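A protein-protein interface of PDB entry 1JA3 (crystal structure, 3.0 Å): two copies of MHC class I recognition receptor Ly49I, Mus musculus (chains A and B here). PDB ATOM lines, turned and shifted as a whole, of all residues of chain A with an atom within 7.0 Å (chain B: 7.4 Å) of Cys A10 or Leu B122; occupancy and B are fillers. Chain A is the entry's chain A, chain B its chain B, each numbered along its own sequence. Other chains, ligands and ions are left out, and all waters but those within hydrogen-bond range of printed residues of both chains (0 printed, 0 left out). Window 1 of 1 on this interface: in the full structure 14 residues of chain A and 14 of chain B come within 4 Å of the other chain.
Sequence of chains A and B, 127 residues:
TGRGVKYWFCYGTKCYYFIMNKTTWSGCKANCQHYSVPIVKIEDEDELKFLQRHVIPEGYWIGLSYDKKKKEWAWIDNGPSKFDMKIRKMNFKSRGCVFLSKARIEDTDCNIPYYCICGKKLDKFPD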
ATOM      1  N   TRP A   8     -12.174  -9.849   0.974  1.00  0.00           N
ATOM      2  CA  TRP A   8     -11.978  -8.575   0.289  1.00  0.00           C
ATOM      3  C   TRP A   8     -12.567  -8.518  -1.102  1.00  0.00           C
ATOM      4  O   TRP A   8     -12.830  -9.537  -1.726  1.00  0.00           O
ATOM      5  CB  TRP A   8     -10.505  -8.208   0.219  1.00  0.00           C
ATOM      6  CG  TRP A   8      -9.693  -9.213  -0.450  1.00  0.00           C
ATOM      7  CD1 TRP A   8      -9.319 -10.419   0.050  1.00  0.00           C
ATOM      8  CD2 TRP A   8      -9.098  -9.106  -1.750  1.00  0.00           C
ATOM      9  NE1 TRP A   8      -8.519 -11.073  -0.855  1.00  0.00           N
ATOM     10  CE2 TRP A   8      -8.369 -10.290  -1.969  1.00  0.00           C
ATOM     11  CE3 TRP A   8      -9.116  -8.125  -2.750  1.00  0.00           C
ATOM     12  CZ2 TRP A   8      -7.656 -10.519  -3.145  1.00  0.00           C
ATOM     13  CZ3 TRP A   8      -8.411  -8.353  -3.914  1.00  0.00           C
ATOM     14  CH2 TRP A   8      -7.691  -9.544  -4.104  1.00  0.00           C
ATOM     15  N   PHE A   9     -12.800  -7.305  -1.572  1.00  0.00           N
ATOM     16  CA  PHE A   9     -13.360  -7.109  -2.885  1.00  0.00           C
ATOM     17  C   PHE A   9     -12.837  -5.821  -3.468  1.00  0.00           C
ATOM     18  O   PHE A   9     -12.257  -5.001  -2.747  1.00  0.00           O
ATOM     19  CB  PHE A   9     -14.879  -7.070  -2.823  1.00  0.00           C
ATOM     20  CG  PHE A   9     -15.530  -8.102  -3.688  1.00  0.00           C
ATOM     21  CD1 PHE A   9     -15.110  -9.439  -3.620  1.00  0.00           C
ATOM     22  CD2 PHE A   9     -16.565  -7.757  -4.566  1.00  0.00           C
ATOM     23  CE1 PHE A   9     -15.711 -10.422  -4.409  1.00  0.00           C
ATOM     24  CE2 PHE A   9     -17.175  -8.736  -5.362  1.00  0.00           C
ATOM     25  CZ  PHE A   9     -16.746 -10.074  -5.281  1.00  0.00           C
ATOM     26  N   CYS A  10     -13.037  -5.646  -4.774  1.00  0.00           N
ATOM     27  CA  CYS A  10     -12.581  -4.451  -5.464  1.00  0.00           C
ATOM     28  C   CYS A  10     -13.659  -3.930  -6.405  1.00  0.00           C
ATOM     29  O   CYS A  10     -14.168  -4.668  -7.249  1.00  0.00           O
ATOM     30  CB  CYS A  10     -11.318  -4.772  -6.251  1.00  0.00           C
ATOM     31  SG  CYS A  10     -10.001  -5.548  -5.262  1.00  0.00           S
ATOM     32  N   TYR A  11     -14.018  -2.662  -6.242  1.00  0.00           N
ATOM     33  CA  TYR A  11     -15.014  -2.036  -7.092  1.00  0.00           C
ATOM     34  C   TYR A  11     -14.430  -0.723  -7.577  1.00  0.00           C
ATOM     35  O   TYR A  11     -14.124   0.158  -6.776  1.00  0.00           O
ATOM     36  CB  TYR A  11     -16.292  -1.775  -6.323  1.00  0.00           C
ATOM     37  CG  TYR A  11     -17.428  -1.365  -7.211  1.00  0.00           C
ATOM     38  CD1 TYR A  11     -17.852  -2.192  -8.246  1.00  0.00           C
ATOM     39  CD2 TYR A  11     -18.074  -0.145  -7.030  1.00  0.00           C
ATOM     40  CE1 TYR A  11     -18.897  -1.814  -9.090  1.00  0.00           C
ATOM     41  CE2 TYR A  11     -19.121   0.256  -7.863  1.00  0.00           C
ATOM     42  CZ  TYR A  11     -19.530  -0.584  -8.901  1.00  0.00           C
ATOM     43  OH  TYR A  11     -20.540  -0.189  -9.762  1.00  0.00           O
ATOM     44  N   GLY A  12     -14.273  -0.601  -8.895  1.00  0.00           N
ATOM     45  CA  GLY A  12     -13.688   0.599  -9.473  1.00  0.00           C
ATOM     46  C   GLY A  12     -12.176   0.563  -9.297  1.00  0.00           C
ATOM     47  O   GLY A  12     -11.556  -0.459  -9.594  1.00  0.00           O
ATOM     48  N   THR A  13     -11.581   1.662  -8.831  1.00  0.00           N
ATOM     49  CA  THR A  13     -10.143   1.698  -8.595  1.00  0.00           C
ATOM     50  C   THR A  13      -9.853   1.440  -7.134  1.00  0.00           C
ATOM     51  O   THR A  13      -8.705   1.479  -6.706  1.00  0.00           O
ATOM     52  CB  THR A  13      -9.520   3.035  -8.926  1.00  0.00           C
ATOM     53  OG1 THR A  13     -10.274   4.070  -8.294  1.00  0.00           O
ATOM     54  CG2 THR A  13      -9.457   3.231 -10.421  1.00  0.00           C
ATOM     55  N   LYS A  14     -10.895   1.182  -6.360  1.00  0.00           N
ATOM     56  CA  LYS A  14     -10.693   0.894  -4.956  1.00  0.00           C
ATOM     57  C   LYS A  14     -10.998  -0.554  -4.565  1.00  0.00           C
ATOM     58  O   LYS A  14     -11.930  -1.170  -5.078  1.00  0.00           O
ATOM     59  CB  LYS A  14     -11.515   1.857  -4.112  1.00  0.00           C
ATOM     60  CG  LYS A  14     -10.809   3.179  -3.869  1.00  0.00           C
ATOM     61  CD  LYS A  14     -11.641   4.082  -2.984  1.00  0.00           C
ATOM     62  CE  LYS A  14     -12.114   3.350  -1.743  1.00  0.00           C
ATOM     63  NZ  LYS A  14     -12.805   4.265  -0.803  1.00  0.00           N
ATOM     64  N   CYS A  15     -10.166  -1.100  -3.683  1.00  0.00           N
ATOM     65  CA  CYS A  15     -10.342  -2.454  -3.179  1.00  0.00           C
ATOM     66  C   CYS A  15     -10.675  -2.275  -1.714  1.00  0.00           C
ATOM     67  O   CYS A  15     -10.149  -1.383  -1.054  1.00  0.00           O
ATOM     68  CB  CYS A  15      -9.064  -3.298  -3.305  1.00  0.00           C
ATOM     69  SG  CYS A  15      -8.652  -4.031  -4.939  1.00  0.00           S
ATOM     70  N   TYR A  16     -11.559  -3.127  -1.219  1.00  0.00           N
ATOM     71  CA  TYR A  16     -11.996  -3.063   0.167  1.00  0.00           C
ATOM     72  C   TYR A  16     -11.680  -4.362   0.887  1.00  0.00           C
ATOM     73  O   TYR A  16     -11.175  -5.319   0.303  1.00  0.00           O
ATOM     74  CB  TYR A  16     -13.512  -2.813   0.249  1.00  0.00           C
ATOM     75  CG  TYR A  16     -14.032  -1.675  -0.614  1.00  0.00           C
ATOM     76  CD1 TYR A  16     -13.953  -1.740  -1.997  1.00  0.00           C
ATOM     77  CD2 TYR A  16     -14.568  -0.521  -0.041  1.00  0.00           C
ATOM     78  CE1 TYR A  16     -14.381  -0.692  -2.793  1.00  0.00           C
ATOM     79  CE2 TYR A  16     -15.002   0.534  -0.838  1.00  0.00           C
ATOM     80  CZ  TYR A  16     -14.903   0.440  -2.217  1.00  0.00           C
ATOM     81  OH  TYR A  16     -15.326   1.474  -3.024  1.00  0.00           O
ATOM     82  N   PHE A  18     -13.671  -6.557   4.096  1.00  0.00           N
ATOM     83  CA  PHE A  18     -14.784  -6.480   5.021  1.00  0.00           C
ATOM     84  C   PHE A  18     -14.496  -7.394   6.185  1.00  0.00           C
ATOM     85  O   PHE A  18     -14.520  -8.615   6.041  1.00  0.00           O
ATOM     86  CB  PHE A  18     -16.092  -6.849   4.331  1.00  0.00           C
ATOM     87  CG  PHE A  18     -16.450  -5.930   3.220  1.00  0.00           C
ATOM     88  CD1 PHE A  18     -15.630  -5.828   2.110  1.00  0.00           C
ATOM     89  CD2 PHE A  18     -17.584  -5.143   3.291  1.00  0.00           C
ATOM     90  CE1 PHE A  18     -15.945  -4.965   1.084  1.00  0.00           C
ATOM     91  CE2 PHE A  18     -17.911  -4.266   2.259  1.00  0.00           C
ATOM     92  CZ  PHE A  18     -17.091  -4.173   1.159  1.00  0.00           C
ATOM     93  N   PHE A  50     -22.642   1.031  -3.582  1.00  0.00           N
ATOM     94  CA  PHE A  50     -21.960  -0.249  -3.788  1.00  0.00           C
ATOM     95  C   PHE A  50     -21.654  -0.962  -2.469  1.00  0.00           C
ATOM     96  O   PHE A  50     -21.823  -2.171  -2.364  1.00  0.00           O
ATOM     97  CB  PHE A  50     -20.649  -0.085  -4.561  1.00  0.00           C
ATOM     98  CG  PHE A  50     -19.769  -1.293  -4.481  1.00  0.00           C
ATOM     99  CD1 PHE A  50     -20.117  -2.459  -5.135  1.00  0.00           C
ATOM    100  CD2 PHE A  50     -18.642  -1.294  -3.675  1.00  0.00           C
ATOM    101  CE1 PHE A  50     -19.361  -3.615  -4.989  1.00  0.00           C
ATOM    102  CE2 PHE A  50     -17.871  -2.440  -3.514  1.00  0.00           C
ATOM    103  CZ  PHE A  50     -18.231  -3.610  -4.176  1.00  0.00           C
ATOM    104  N   LEU A 122      -6.247   2.598  -5.564  1.00  0.00           N
ATOM    105  CA  LEU A 122      -5.310   1.925  -6.435  1.00  0.00           C
ATOM    106  C   LEU A 122      -4.652   2.972  -7.321  1.00  0.00           C
ATOM    107  O   LEU A 122      -5.178   4.073  -7.509  1.00  0.00           O
ATOM    108  CB  LEU A 122      -6.036   0.858  -7.268  1.00  0.00           C
ATOM    109  CG  LEU A 122      -6.154  -0.567  -6.691  1.00  0.00           C
ATOM    110  CD1 LEU A 122      -6.870  -0.607  -5.360  1.00  0.00           C
ATOM    111  CD2 LEU A 122      -6.900  -1.408  -7.679  1.00  0.00           C
ATOM    112  N   PHE A 125      -2.723  -1.480 -11.299  1.00  0.00           N
ATOM    113  CA  PHE A 125      -3.531  -2.565 -11.757  1.00  0.00           C
ATOM    114  C   PHE A 125      -2.946  -3.767 -11.010  1.00  0.00           C
ATOM    115  O   PHE A 125      -3.691  -4.495 -10.341  1.00  0.00           O
ATOM    116  CB  PHE A 125      -3.370  -2.719 -13.280  1.00  0.00           C
ATOM    117  CG  PHE A 125      -4.546  -3.373 -13.960  1.00  0.00           C
ATOM    118  CD1 PHE A 125      -5.632  -2.616 -14.369  1.00  0.00           C
ATOM    119  CD2 PHE A 125      -4.587  -4.754 -14.154  1.00  0.00           C
ATOM    120  CE1 PHE A 125      -6.744  -3.221 -14.965  1.00  0.00           C
ATOM    121  CE2 PHE A 125      -5.697  -5.368 -14.750  1.00  0.00           C
ATOM    122  CZ  PHE A 125      -6.775  -4.599 -15.150  1.00  0.00           C
ATOM    123  N   PRO A 126      -1.591  -3.953 -11.064  1.00  0.00           N
ATOM    124  CA  PRO A 126      -0.924  -5.084 -10.387  1.00  0.00           C
ATOM    125  C   PRO A 126      -1.166  -5.113  -8.873  1.00  0.00           C
ATOM    126  O   PRO A 126      -1.785  -4.141  -8.359  1.00  0.00           O
ATOM    127  CB  PRO A 126       0.555  -4.870 -10.723  1.00  0.00           C
ATOM    128  CG  PRO A 126       0.651  -3.379 -10.724  1.00  0.00           C
ATOM    129  CD  PRO A 126      -0.572  -2.995 -11.548  1.00  0.00           C
ATOM    130  N   PHE B   9     -10.694  -1.123 -14.773  1.00  0.00           N
ATOM    131  CA  PHE B   9     -11.675  -1.146 -13.702  1.00  0.00           C
ATOM    132  C   PHE B   9     -11.574  -2.467 -12.990  1.00  0.00           C
ATOM    133  O   PHE B   9     -11.147  -3.457 -13.573  1.00  0.00           O
ATOM    134  CB  PHE B   9     -13.086  -0.984 -14.267  1.00  0.00           C
ATOM    135  CG  PHE B   9     -13.914   0.027 -13.534  1.00  0.00           C
ATOM    136  CD1 PHE B   9     -13.537   1.371 -13.532  1.00  0.00           C
ATOM    137  CD2 PHE B   9     -15.061  -0.360 -12.832  1.00  0.00           C
ATOM    138  CE1 PHE B   9     -14.276   2.324 -12.844  1.00  0.00           C
ATOM    139  CE2 PHE B   9     -15.816   0.586 -12.138  1.00  0.00           C
ATOM    140  CZ  PHE B   9     -15.420   1.937 -12.145  1.00  0.00           C
ATOM    141  N   CYS B  10     -11.970  -2.495 -11.727  1.00  0.00           N
ATOM    142  CA  CYS B  10     -11.898  -3.736 -10.993  1.00  0.00           C
ATOM    143  C   CYS B  10     -13.266  -4.071 -10.431  1.00  0.00           C
ATOM    144  O   CYS B  10     -14.055  -3.186 -10.105  1.00  0.00           O
ATOM    145  CB  CYS B  10     -10.846  -3.643  -9.879  1.00  0.00           C
ATOM    146  SG  CYS B  10      -9.191  -3.044 -10.402  1.00  0.00           S
ATOM    147  N   TYR B  11     -13.544  -5.368 -10.377  1.00  0.00           N
ATOM    148  CA  TYR B  11     -14.794  -5.906  -9.872  1.00  0.00           C
ATOM    149  C   TYR B  11     -14.370  -7.212  -9.240  1.00  0.00           C
ATOM    150  O   TYR B  11     -13.514  -7.901  -9.784  1.00  0.00           O
ATOM    151  CB  TYR B  11     -15.770  -6.176 -11.021  1.00  0.00           C
ATOM    152  CG  TYR B  11     -17.153  -6.541 -10.556  1.00  0.00           C
ATOM    153  CD1 TYR B  11     -17.882  -5.672  -9.745  1.00  0.00           C
ATOM    154  CD2 TYR B  11     -17.721  -7.766 -10.886  1.00  0.00           C
ATOM    155  CE1 TYR B  11     -19.145  -6.016  -9.264  1.00  0.00           C
ATOM    156  CE2 TYR B  11     -18.988  -8.126 -10.412  1.00  0.00           C
ATOM    157  CZ  TYR B  11     -19.691  -7.244  -9.597  1.00  0.00           C
ATOM    158  OH  TYR B  11     -20.924  -7.603  -9.099  1.00  0.00           O
ATOM    159  N   GLY B  12     -14.938  -7.557  -8.096  1.00  0.00           N
ATOM    160  CA  GLY B  12     -14.532  -8.799  -7.477  1.00  0.00           C
ATOM    161  C   GLY B  12     -13.022  -8.835  -7.374  1.00  0.00           C
ATOM    162  O   GLY B  12     -12.402  -7.792  -7.218  1.00  0.00           O
ATOM    163  N   THR B  13     -12.423 -10.012  -7.482  1.00  0.00           N
ATOM    164  CA  THR B  13     -10.978 -10.127  -7.372  1.00  0.00           C
ATOM    165  C   THR B  13     -10.195  -9.934  -8.673  1.00  0.00           C
ATOM    166  O   THR B  13      -9.033 -10.332  -8.783  1.00  0.00           O
ATOM    167  CB  THR B  13     -10.598 -11.477  -6.762  1.00  0.00           C
ATOM    168  OG1 THR B  13     -11.288 -12.530  -7.453  1.00  0.00           O
ATOM    169  CG2 THR B  13     -10.962 -11.500  -5.296  1.00  0.00           C
ATOM    170  N   LYS B  14     -10.816  -9.311  -9.658  1.00  0.00           N
ATOM    171  CA  LYS B  14     -10.131  -9.103 -10.919  1.00  0.00           C
ATOM    172  C   LYS B  14     -10.286  -7.679 -11.382  1.00  0.00           C
ATOM    173  O   LYS B  14     -11.247  -6.993 -11.050  1.00  0.00           O
ATOM    174  CB  LYS B  14     -10.687 -10.019 -12.015  1.00  0.00           C
ATOM    175  CG  LYS B  14     -10.506 -11.498 -11.798  1.00  0.00           C
ATOM    176  CD  LYS B  14     -11.222 -12.287 -12.892  1.00  0.00           C
ATOM    177  CE  LYS B  14     -10.736 -11.918 -14.296  1.00  0.00           C
ATOM    178  NZ  LYS B  14     -11.202 -12.890 -15.340  1.00  0.00           N
ATOM    179  N   CYS B  15      -9.325  -7.246 -12.172  1.00  0.00           N
ATOM    180  CA  CYS B  15      -9.352  -5.916 -12.722  1.00  0.00           C
ATOM    181  C   CYS B  15      -9.390  -6.123 -14.215  1.00  0.00           C
ATOM    182  O   CYS B  15      -8.960  -7.174 -14.717  1.00  0.00           O
ATOM    183  CB  CYS B  15      -8.103  -5.133 -12.331  1.00  0.00           C
ATOM    184  SG  CYS B  15      -8.009  -4.689 -10.573  1.00  0.00           S
ATOM    185  N   TYR B  16      -9.911  -5.118 -14.919  1.00  0.00           N
ATOM    186  CA  TYR B  16     -10.039  -5.174 -16.360  1.00  0.00           C
ATOM    187  C   TYR B  16      -9.459  -3.958 -17.031  1.00  0.00           C
ATOM    188  O   TYR B  16      -9.309  -2.903 -16.417  1.00  0.00           O
ATOM    189  CB  TYR B  16     -11.506  -5.296 -16.748  1.00  0.00           C
ATOM    190  CG  TYR B  16     -12.233  -6.391 -16.022  1.00  0.00           C
ATOM    191  CD1 TYR B  16     -12.579  -6.244 -14.683  1.00  0.00           C
ATOM    192  CD2 TYR B  16     -12.531  -7.593 -16.659  1.00  0.00           C
ATOM    193  CE1 TYR B  16     -13.192  -7.264 -13.991  1.00  0.00           C
ATOM    194  CE2 TYR B  16     -13.148  -8.622 -15.976  1.00  0.00           C
ATOM    195  CZ  TYR B  16     -13.474  -8.461 -14.637  1.00  0.00           C
ATOM    196  OH  TYR B  16     -14.030  -9.507 -13.926  1.00  0.00           O
ATOM    197  N   PHE B  50     -21.329  -9.044 -15.515  1.00  0.00           N
ATOM    198  CA  PHE B  50     -20.756  -7.785 -15.070  1.00  0.00           C
ATOM    199  C   PHE B  50     -20.200  -6.960 -16.194  1.00  0.00           C
ATOM    200  O   PHE B  50     -20.417  -5.761 -16.239  1.00  0.00           O
ATOM    201  CB  PHE B  50     -19.620  -7.949 -14.084  1.00  0.00           C
ATOM    202  CG  PHE B  50     -18.917  -6.661 -13.831  1.00  0.00           C
ATOM    203  CD1 PHE B  50     -19.548  -5.664 -13.104  1.00  0.00           C
ATOM    204  CD2 PHE B  50     -17.679  -6.396 -14.410  1.00  0.00           C
ATOM    205  CE1 PHE B  50     -18.971  -4.416 -12.965  1.00  0.00           C
ATOM    206  CE2 PHE B  50     -17.084  -5.148 -14.280  1.00  0.00           C
ATOM    207  CZ  PHE B  50     -17.729  -4.154 -13.554  1.00  0.00           C
ATOM    208  N   LYS B 120      -6.593  -9.076 -15.548  1.00  0.00           N
ATOM    209  CA  LYS B 120      -5.655  -9.787 -14.690  1.00  0.00           C
ATOM    210  C   LYS B 120      -6.343 -10.290 -13.426  1.00  0.00           C
ATOM    211  O   LYS B 120      -7.295  -9.630 -12.988  1.00  0.00           O
ATOM    212  CB  LYS B 120      -4.484  -8.875 -14.314  1.00  0.00           C
ATOM    213  CG  LYS B 120      -4.182  -8.833 -12.825  1.00  0.00           C
ATOM    214  CD  LYS B 120      -2.684  -8.797 -12.567  1.00  0.00           C
ATOM    215  CE  LYS B 120      -1.966  -9.887 -13.346  1.00  0.00           C
ATOM    216  NZ  LYS B 120      -0.497  -9.864 -13.103  1.00  0.00           N
ATOM    217  N   LYS B 121      -5.897 -11.383 -12.891  1.00  0.00           N
ATOM    218  CA  LYS B 121      -6.493 -11.913 -11.671  1.00  0.00           C
ATOM    219  C   LYS B 121      -5.757 -11.247 -10.502  1.00  0.00           C
ATOM    220  O   LYS B 121      -4.635 -10.751 -10.661  1.00  0.00           O
ATOM    221  CB  LYS B 121      -6.291 -13.429 -11.620  1.00  0.00           C
ATOM    222  CG  LYS B 121      -7.067 -14.142 -10.543  1.00  0.00           C
ATOM    223  CD  LYS B 121      -8.529 -14.134 -10.869  1.00  0.00           C
ATOM    224  CE  LYS B 121      -9.296 -15.070  -9.954  1.00  0.00           C
ATOM    225  NZ  LYS B 121     -10.773 -15.009 -10.225  1.00  0.00           N
ATOM    226  N   LEU B 122      -6.376 -11.215  -9.334  1.00  0.00           N
ATOM    227  CA  LEU B 122      -5.715 -10.605  -8.198  1.00  0.00           C
ATOM    228  C   LEU B 122      -5.408 -11.680  -7.180  1.00  0.00           C
ATOM    229  O   LEU B 122      -6.178 -12.629  -7.027  1.00  0.00           O
ATOM    230  CB  LEU B 122      -6.601  -9.512  -7.602  1.00  0.00           C
ATOM    231  CG  LEU B 122      -6.210  -8.056  -7.929  1.00  0.00           C
ATOM    232  CD1 LEU B 122      -5.755  -7.887  -9.371  1.00  0.00           C
ATOM    233  CD2 LEU B 122      -7.395  -7.161  -7.663  1.00  0.00           C
ATOM    234  N   ASP B 123      -4.263 -11.547  -6.508  1.00  0.00           N
ATOM    235  CA  ASP B 123      -3.828 -12.510  -5.483  1.00  0.00           C
ATOM    236  C   ASP B 123      -3.564 -11.802  -4.167  1.00  0.00           C
ATOM    237  O   ASP B 123      -3.428 -12.447  -3.128  1.00  0.00           O
ATOM    238  CB  ASP B 123      -2.531 -13.207  -5.892  1.00  0.00           C
ATOM    239  CG  ASP B 123      -2.548 -13.657  -7.325  1.00  0.00           C
ATOM    240  OD1 ASP B 123      -3.489 -14.408  -7.678  1.00  0.00           O
ATOM    241  OD2 ASP B 123      -1.632 -13.263  -8.090  1.00  0.00           O
ATOM    242  N   LYS B 124      -3.484 -10.479  -4.209  1.00  0.00           N
ATOM    243  CA  LYS B 124      -3.197  -9.718  -3.005  1.00  0.00           C
ATOM    244  C   LYS B 124      -4.212  -8.641  -2.703  1.00  0.00           C
ATOM    245  O   LYS B 124      -5.368  -8.918  -2.377  1.00  0.00           O
ATOM    246  CB  LYS B 124      -1.805  -9.082  -3.103  1.00  0.00           C
ATOM    247  CG  LYS B 124      -0.632 -10.055  -2.913  1.00  0.00           C
ATOM    248  CD  LYS B 124       0.071  -9.822  -1.562  1.00  0.00           C
ATOM    249  CE  LYS B 124      -0.168 -10.951  -0.559  1.00  0.00           C
ATOM    250  NZ  LYS B 124      -1.604 -11.128  -0.218  1.00  0.00           N
ATOM    251  N   PHE B 125      -3.759  -7.400  -2.791  1.00  0.00           N
ATOM    252  CA  PHE B 125      -4.630  -6.282  -2.518  1.00  0.00           C
ATOM    253  C   PHE B 125      -4.054  -5.087  -3.262  1.00  0.00           C
ATOM    254  O   PHE B 125      -4.699  -4.703  -4.258  1.00  0.00           O
ATOM    255  CB  PHE B 125      -4.702  -6.017  -0.998  1.00  0.00           C
ATOM    256  CG  PHE B 125      -5.936  -5.264  -0.573  1.00  0.00           C
ATOM    257  CD1 PHE B 125      -7.063  -5.941  -0.131  1.00  0.00           C
ATOM    258  CD2 PHE B 125      -5.998  -3.879  -0.692  1.00  0.00           C
ATOM    259  CE1 PHE B 125      -8.235  -5.249   0.177  1.00  0.00           C
ATOM    260  CE2 PHE B 125      -7.166  -3.184  -0.387  1.00  0.00           C
ATOM    261  CZ  PHE B 125      -8.283  -3.871   0.045  1.00  0.00           C
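N of Tyr A16 lies within hydrogen-bond range of O of Phe A9 (2.5 Å).
The side-chain sulfur of Cys A10 forms a disulfide with the side-chain sulfur of Cys A15.
O of Phe B9 lies within hydrogen-bond range of N of Tyr B16, 2.5 Å away.
SG of Cys B10 forms a disulfide with SG of Cys B15.
The backbone carbonyl oxygen (O) of Thr B13 sits close to the backbone NH (N) of Leu B122.
The backbone NH of Lys B120 is in hydrogen-bond range of the backbone carbonyl oxygen of Cys B15.
O of Cys A10 lies close to N of Tyr B11, at 3.3 Å.
The backbone NH (N) of Gly B12 sits at hydrogen-bond distance from the backbone carbonyl oxygen (O) of Cys A10 (3.1 Å).
O of Cys B10 is in hydrogen-bond range of N of Gly A12.
The backbone carbonyl oxygen (O) of Cys A10 lies close to the backbone carbonyl oxygen (O) of Cys B10.
Cys A10 touches Tyr B11, and with the chains exchanged Tyr A11 touches Cys B10.
Cys A10 touches Gly B12, and with the chains exchanged Gly A12 touches Cys B10.
Tyr B11 touches its own counterpart, Tyr A11.
Tyr A16 touches Phe B125, and with the chains exchanged Phe A125 touches Tyr B16.
Among the printed residues, merely in contact across the chains: Trp A8 with Lys B124, Tyr A16 with Phe B125, Phe A125 with Tyr B16, Phe A125 with Cys B15, Cys A15 with Phe B125, Tyr A11 with Cys B10, Phe A9 with Gly B12, Gly A12 with Phe B9, Trp A8 with Leu B122, Trp A8 with Phe B125, Phe A125 with Lys B120, Tyr A11 with Tyr B11, Cys A10 with Leu B122, Leu A122 with Cys B10 and Trp A8 with Thr B13.
Cys A10 touches just these residues of chain B: Cys B10, Tyr B11, Gly B12 and Leu B122.
Of the printed residues of chain A, Phe B9 touches Gly A12 (3.4 Å).
Of the printed residues of chain A, Tyr B16 touches Phe A125 (3.0 Å).
Printed residues of chain A within 4 Å of Leu B122: Trp A8 and Cys A10.
Asp B123 touches none of the printed residues of chain A.
The nearest residue of chain A that does not touch Leu B122 is Phe A125 (4.1 Å).
The nearest printed residue of chain A that does not touch Cys B10 is Thr A13 (5.1 Å).
Of the 15 printed residues of chain B, 11 touch a printed residue of chain A.
Hydrophobic or aromatic side chains of chain B that line the printed part of chain A: Phe B9, Tyr B11, Leu B122 and Phe B125.
Among the printed residues, 19 pairs touch across the chains.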
